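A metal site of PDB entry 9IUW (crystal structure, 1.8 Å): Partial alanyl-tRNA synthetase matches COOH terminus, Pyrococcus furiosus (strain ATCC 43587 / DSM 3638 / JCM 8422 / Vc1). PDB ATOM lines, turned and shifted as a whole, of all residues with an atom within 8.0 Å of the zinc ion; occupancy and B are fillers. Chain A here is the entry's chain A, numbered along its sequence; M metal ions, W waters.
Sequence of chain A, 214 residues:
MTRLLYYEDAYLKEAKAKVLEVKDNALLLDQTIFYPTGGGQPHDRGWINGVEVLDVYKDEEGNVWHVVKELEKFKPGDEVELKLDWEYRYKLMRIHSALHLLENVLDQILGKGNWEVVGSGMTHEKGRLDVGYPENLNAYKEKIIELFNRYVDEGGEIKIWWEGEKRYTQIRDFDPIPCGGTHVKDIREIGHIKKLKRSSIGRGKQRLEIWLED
Water W2 is bound to the zinc ion.
The zinc ion is bound by NE2 of His 100, 2.2 Å away.
A ring nitrogen (NE2) of His 96 is bound to the zinc ion, 2.2 Å away.
Water W1 binds the zinc ion.
The zinc ion is bound by SG of Cys 179, 2.3 Å away.
The zinc ion has five donor atoms within binding distance.
Water W1 bridges O of Gly 39 (2.8 Å) and O of Gly 180 (3.3 Å).
The side-chain hydroxyl (OG1) of Thr 169 lies within hydrogen-bond range of a ring nitrogen (ND1) of His 100 (2.9 Å).
OE1 of Gln 41 lies within hydrogen-bond range of ND1 of His 96 (2.7 Å).
The backbone NH (N) of Cys 179 sits at hydrogen-bond distance from the backbone carbonyl oxygen (O) of Arg 167 (2.7 Å).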
ATOM      1  N   TYR A  35     -21.613  20.105 -35.342  1.00  0.00           N
ATOM      2  CA  TYR A  35     -20.833  20.885 -34.383  1.00  0.00           C
ATOM      3  C   TYR A  35     -19.418  20.317 -34.274  1.00  0.00           C
ATOM      4  O   TYR A  35     -19.258  19.114 -34.000  1.00  0.00           O
ATOM      5  CB  TYR A  35     -21.533  20.883 -33.028  1.00  0.00           C
ATOM      6  CG  TYR A  35     -20.787  21.664 -31.962  1.00  0.00           C
ATOM      7  CD1 TYR A  35     -20.845  23.052 -31.937  1.00  0.00           C
ATOM      8  CD2 TYR A  35     -20.035  21.005 -31.003  1.00  0.00           C
ATOM      9  CE1 TYR A  35     -20.160  23.773 -30.970  1.00  0.00           C
ATOM     10  CE2 TYR A  35     -19.348  21.712 -30.042  1.00  0.00           C
ATOM     11  CZ  TYR A  35     -19.414  23.086 -30.022  1.00  0.00           C
ATOM     12  OH  TYR A  35     -18.727  23.794 -29.061  1.00  0.00           O
ATOM     13  N   GLY A  38     -15.311  21.580 -29.365  1.00  0.00           N
ATOM     14  CA  GLY A  38     -14.862  22.833 -28.759  1.00  0.00           C
ATOM     15  C   GLY A  38     -15.705  23.188 -27.559  1.00  0.00           C
ATOM     16  O   GLY A  38     -16.851  22.750 -27.417  1.00  0.00           O
ATOM     17  N   GLY A  39     -15.107  23.997 -26.671  1.00  0.00           N
ATOM     18  CA  GLY A  39     -15.844  24.501 -25.528  1.00  0.00           C
ATOM     19  C   GLY A  39     -16.230  23.459 -24.505  1.00  0.00           C
ATOM     20  O   GLY A  39     -17.167  23.688 -23.717  1.00  0.00           O
ATOM     21  N   GLY A  40     -15.546  22.321 -24.491  1.00  0.00           N
ATOM     22  CA  GLY A  40     -15.896  21.188 -23.655  1.00  0.00           C
ATOM     23  C   GLY A  40     -16.978  20.283 -24.212  1.00  0.00           C
ATOM     24  O   GLY A  40     -17.260  19.241 -23.606  1.00  0.00           O
ATOM     25  N   GLN A  41     -17.613  20.653 -25.353  1.00  0.00           N
ATOM     26  CA  GLN A  41     -18.675  19.860 -25.957  1.00  0.00           C
ATOM     27  C   GLN A  41     -18.103  19.014 -27.096  1.00  0.00           C
ATOM     28  O   GLN A  41     -17.487  19.567 -28.009  1.00  0.00           O
ATOM     29  CB  GLN A  41     -19.789  20.757 -26.502  1.00  0.00           C
ATOM     30  CG  GLN A  41     -21.029  19.998 -26.994  1.00  0.00           C
ATOM     31  CD  GLN A  41     -22.081  20.901 -27.613  1.00  0.00           C
ATOM     32  OE1 GLN A  41     -22.335  22.003 -27.128  1.00  0.00           O
ATOM     33  NE2 GLN A  41     -22.718  20.425 -28.681  1.00  0.00           N
ATOM     34  N   ILE A  95     -27.233  18.602 -21.571  1.00  0.00           N
ATOM     35  CA  ILE A  95     -26.169  18.592 -20.573  1.00  0.00           C
ATOM     36  C   ILE A  95     -25.402  19.901 -20.600  1.00  0.00           C
ATOM     37  O   ILE A  95     -25.043  20.452 -19.553  1.00  0.00           O
ATOM     38  CB  ILE A  95     -25.238  17.388 -20.784  1.00  0.00           C
ATOM     39  CG1 ILE A  95     -25.999  16.104 -20.429  1.00  0.00           C
ATOM     40  CG2 ILE A  95     -23.974  17.527 -19.912  1.00  0.00           C
ATOM     41  CD1 ILE A  95     -25.256  14.824 -20.797  1.00  0.00           C
ATOM     42  N   HIS A  96     -25.189  20.451 -21.784  1.00  0.00           N
ATOM     43  CA  HIS A  96     -24.476  21.721 -21.863  1.00  0.00           C
ATOM     44  C   HIS A  96     -25.260  22.818 -21.179  1.00  0.00           C
ATOM     45  O   HIS A  96     -24.725  23.584 -20.376  1.00  0.00           O
ATOM     46  CB  HIS A  96     -24.202  22.069 -23.316  1.00  0.00           C
ATOM     47  CG  HIS A  96     -23.070  23.019 -23.485  1.00  0.00           C
ATOM     48  ND1 HIS A  96     -22.359  23.136 -24.660  1.00  0.00           N
ATOM     49  CD2 HIS A  96     -22.509  23.893 -22.617  1.00  0.00           C
ATOM     50  CE1 HIS A  96     -21.414  24.042 -24.518  1.00  0.00           C
ATOM     51  NE2 HIS A  96     -21.486  24.523 -23.290  1.00  0.00           N
ATOM     52  N   SER A  97     -26.557  22.899 -21.471  1.00  0.00           N
ATOM     53  CA  SER A  97     -27.372  23.918 -20.810  1.00  0.00           C
ATOM     54  C   SER A  97     -27.467  23.663 -19.307  1.00  0.00           C
ATOM     55  O   SER A  97     -27.505  24.626 -18.537  1.00  0.00           O
ATOM     56  CB  SER A  97     -28.746  23.991 -21.477  1.00  0.00           C
ATOM     57  OG  SER A  97     -28.598  24.362 -22.851  1.00  0.00           O
ATOM     58  N   LEU A  99     -25.034  22.529 -17.438  1.00  0.00           N
ATOM     59  CA  LEU A  99     -23.804  23.071 -16.864  1.00  0.00           C
ATOM     60  C   LEU A  99     -23.881  24.585 -16.676  1.00  0.00           C
ATOM     61  O   LEU A  99     -23.439  25.119 -15.659  1.00  0.00           O
ATOM     62  CB  LEU A  99     -22.590  22.722 -17.730  1.00  0.00           C
ATOM     63  CG  LEU A  99     -22.128  21.275 -17.600  1.00  0.00           C
ATOM     64  CD1 LEU A  99     -21.158  20.942 -18.754  1.00  0.00           C
ATOM     65  CD2 LEU A  99     -21.452  21.016 -16.241  1.00  0.00           C
ATOM     66  N   HIS A 100     -24.477  25.297 -17.646  1.00  0.00           N
ATOM     67  CA  HIS A 100     -24.696  26.729 -17.488  1.00  0.00           C
ATOM     68  C   HIS A 100     -25.651  27.020 -16.335  1.00  0.00           C
ATOM     69  O   HIS A 100     -25.391  27.904 -15.507  1.00  0.00           O
ATOM     70  CB  HIS A 100     -25.249  27.327 -18.776  1.00  0.00           C
ATOM     71  CG  HIS A 100     -24.222  27.473 -19.850  1.00  0.00           C
ATOM     72  ND1 HIS A 100     -24.206  28.548 -20.721  1.00  0.00           N
ATOM     73  CD2 HIS A 100     -23.171  26.694 -20.193  1.00  0.00           C
ATOM     74  CE1 HIS A 100     -23.197  28.411 -21.565  1.00  0.00           C
ATOM     75  NE2 HIS A 100     -22.546  27.300 -21.259  1.00  0.00           N
ATOM     76  N   GLU A 103     -23.947  26.608 -13.078  1.00  0.00           N
ATOM     77  CA  GLU A 103     -23.066  27.763 -12.733  1.00  0.00           C
ATOM     78  C   GLU A 103     -23.903  28.914 -12.141  1.00  0.00           C
ATOM     79  O   GLU A 103     -23.522  29.455 -11.121  1.00  0.00           O
ATOM     80  CB  GLU A 103     -22.274  28.278 -13.943  1.00  0.00           C
ATOM     81  CG  GLU A 103     -21.255  27.278 -14.454  1.00  0.00           C
ATOM     82  CD  GLU A 103     -20.542  27.781 -15.698  1.00  0.00           C
ATOM     83  OE1 GLU A 103     -20.497  27.010 -16.682  1.00  0.00           O
ATOM     84  OE2 GLU A 103     -20.072  28.934 -15.669  1.00  0.00           O
ATOM     85  N   SER A 120     -14.368  22.658 -17.272  1.00  0.00           N
ATOM     86  CA  SER A 120     -15.728  22.343 -17.703  1.00  0.00           C
ATOM     87  C   SER A 120     -15.645  21.369 -18.880  1.00  0.00           C
ATOM     88  O   SER A 120     -14.809  21.552 -19.756  1.00  0.00           O
ATOM     89  CB  SER A 120     -16.483  23.615 -18.120  1.00  0.00           C
ATOM     90  OG  SER A 120     -17.861  23.374 -18.279  1.00  0.00           O
ATOM     91  N   MET A 122     -18.018  17.773 -20.962  1.00  0.00           N
ATOM     92  CA  MET A 122     -19.195  16.910 -20.933  1.00  0.00           C
ATOM     93  C   MET A 122     -19.019  15.756 -21.893  1.00  0.00           C
ATOM     94  O   MET A 122     -18.239  15.814 -22.840  1.00  0.00           O
ATOM     95  CB  MET A 122     -20.464  17.700 -21.291  1.00  0.00           C
ATOM     96  CG  MET A 122     -20.358  18.285 -22.696  1.00  0.00           C
ATOM     97  SD  MET A 122     -21.517  19.624 -22.999  1.00  0.00           S
ATOM     98  CE  MET A 122     -20.426  20.966 -22.599  1.00  0.00           C
ATOM     99  N   ARG A 167     -19.253  33.965 -28.332  1.00  0.00           N
ATOM    100  CA  ARG A 167     -20.710  33.742 -28.286  1.00  0.00           C
ATOM    101  C   ARG A 167     -21.134  33.759 -26.819  1.00  0.00           C
ATOM    102  O   ARG A 167     -20.408  33.203 -25.994  1.00  0.00           O
ATOM    103  CB  ARG A 167     -21.049  32.399 -28.921  1.00  0.00           C
ATOM    104  CG  ARG A 167     -22.511  32.274 -29.323  1.00  0.00           C
ATOM    105  CD  ARG A 167     -22.797  30.876 -29.843  1.00  0.00           C
ATOM    106  NE  ARG A 167     -24.049  30.773 -30.587  1.00  0.00           N
ATOM    107  CZ  ARG A 167     -24.985  29.864 -30.388  1.00  0.00           C
ATOM    108  NH1 ARG A 167     -24.907  29.009 -29.386  1.00  0.00           N
ATOM    109  NH2 ARG A 167     -26.029  29.823 -31.208  1.00  0.00           N
ATOM    110  N   THR A 169     -24.415  33.233 -23.956  1.00  0.00           N
ATOM    111  CA  THR A 169     -25.709  32.628 -23.666  1.00  0.00           C
ATOM    112  C   THR A 169     -26.175  33.174 -22.333  1.00  0.00           C
ATOM    113  O   THR A 169     -25.370  33.466 -21.444  1.00  0.00           O
ATOM    114  CB  THR A 169     -25.640  31.104 -23.577  1.00  0.00           C
ATOM    115  OG1 THR A 169     -24.741  30.746 -22.540  1.00  0.00           O
ATOM    116  CG2 THR A 169     -25.128  30.489 -24.876  1.00  0.00           C
ATOM    117  N   ILE A 177     -23.033  33.770 -19.825  1.00  0.00           N
ATOM    118  CA  ILE A 177     -21.899  32.857 -19.818  1.00  0.00           C
ATOM    119  C   ILE A 177     -21.354  32.719 -21.234  1.00  0.00           C
ATOM    120  O   ILE A 177     -22.059  32.259 -22.130  1.00  0.00           O
ATOM    121  CB  ILE A 177     -22.264  31.475 -19.269  1.00  0.00           C
ATOM    122  CG1 ILE A 177     -22.688  31.592 -17.801  1.00  0.00           C
ATOM    123  CG2 ILE A 177     -21.109  30.509 -19.412  1.00  0.00           C
ATOM    124  CD1 ILE A 177     -23.420  30.361 -17.281  1.00  0.00           C
ATOM    125  N   PRO A 178     -20.119  33.224 -21.541  1.00  0.00           N
ATOM    126  CA  PRO A 178     -19.595  33.176 -22.899  1.00  0.00           C
ATOM    127  C   PRO A 178     -19.016  31.808 -23.209  1.00  0.00           C
ATOM    128  O   PRO A 178     -18.186  31.318 -22.405  1.00  0.00           O
ATOM    129  CB  PRO A 178     -18.500  34.243 -22.947  1.00  0.00           C
ATOM    130  CG  PRO A 178     -17.993  34.323 -21.531  1.00  0.00           C
ATOM    131  CD  PRO A 178     -19.143  33.885 -20.645  1.00  0.00           C
ATOM    132  N   CYS A 179     -19.399  31.242 -24.360  1.00  0.00           N
ATOM    133  CA  CYS A 179     -18.843  29.930 -24.762  1.00  0.00           C
ATOM    134  C   CYS A 179     -19.451  29.438 -26.073  1.00  0.00           C
ATOM    135  O   CYS A 179     -20.573  29.877 -26.409  1.00  0.00           O
ATOM    136  CB  CYS A 179     -19.149  28.877 -23.706  1.00  0.00           C
ATOM    137  SG  CYS A 179     -20.708  28.005 -23.965  1.00  0.00           S
ATOM    138  N   GLY A 180     -18.739  28.554 -26.780  1.00  0.00           N
ATOM    139  CA  GLY A 180     -19.297  27.950 -28.005  1.00  0.00           C
ATOM    140  C   GLY A 180     -20.018  26.670 -27.649  1.00  0.00           C
ATOM    141  O   GLY A 180     -19.702  26.107 -26.580  1.00  0.00           O
ATOM    142  N   GLY A 181     -20.935  26.198 -28.501  1.00  0.00           N
ATOM    143  CA  GLY A 181     -21.707  25.026 -28.163  1.00  0.00           C
ATOM    144  C   GLY A 181     -23.185  25.262 -28.340  1.00  0.00           C
ATOM    145  O   GLY A 181     -23.651  26.387 -28.528  1.00  0.00           O
ATOM    146  N   THR A 182     -23.924  24.158 -28.302  1.00  0.00           N
ATOM    147  CA  THR A 182     -25.326  24.129 -28.697  1.00  0.00           C
ATOM    148  C   THR A 182     -26.176  23.958 -27.445  1.00  0.00           C
ATOM    149  O   THR A 182     -25.897  23.070 -26.632  1.00  0.00           O
ATOM    150  CB  THR A 182     -25.594  22.995 -29.691  1.00  0.00           C
ATOM    151  OG1 THR A 182     -25.201  21.761 -29.090  1.00  0.00           O
ATOM    152  CG2 THR A 182     -24.809  23.216 -30.992  1.00  0.00           C
ATOM    153  N   HIS A 183     -27.195  24.791 -27.309  1.00  0.00           N
ATOM    154  CA  HIS A 183     -28.016  24.841 -26.107  1.00  0.00           C
ATOM    155  C   HIS A 183     -29.466  24.589 -26.452  1.00  0.00           C
ATOM    156  O   HIS A 183     -29.904  24.804 -27.587  1.00  0.00           O
ATOM    157  CB  HIS A 183     -27.861  26.193 -25.414  1.00  0.00           C
ATOM    158  CG  HIS A 183     -26.534  26.362 -24.736  1.00  0.00           C
ATOM    159  ND1 HIS A 183     -26.313  25.958 -23.438  1.00  0.00           N
ATOM    160  CD2 HIS A 183     -25.354  26.854 -25.183  1.00  0.00           C
ATOM    161  CE1 HIS A 183     -25.059  26.173 -23.113  1.00  0.00           C
ATOM    162  NE2 HIS A 183     -24.450  26.735 -24.151  1.00  0.00           N
HETATM  163 ZN    ZN M   1     -20.774  26.388 -22.273  1.00  0.00          ZN
HETATM  164  O   HOH W   1     -18.791  25.993 -23.429  1.00  0.00           O
HETATM  165  O   HOH W   2     -20.054  25.309 -20.521  1.00  0.00           O
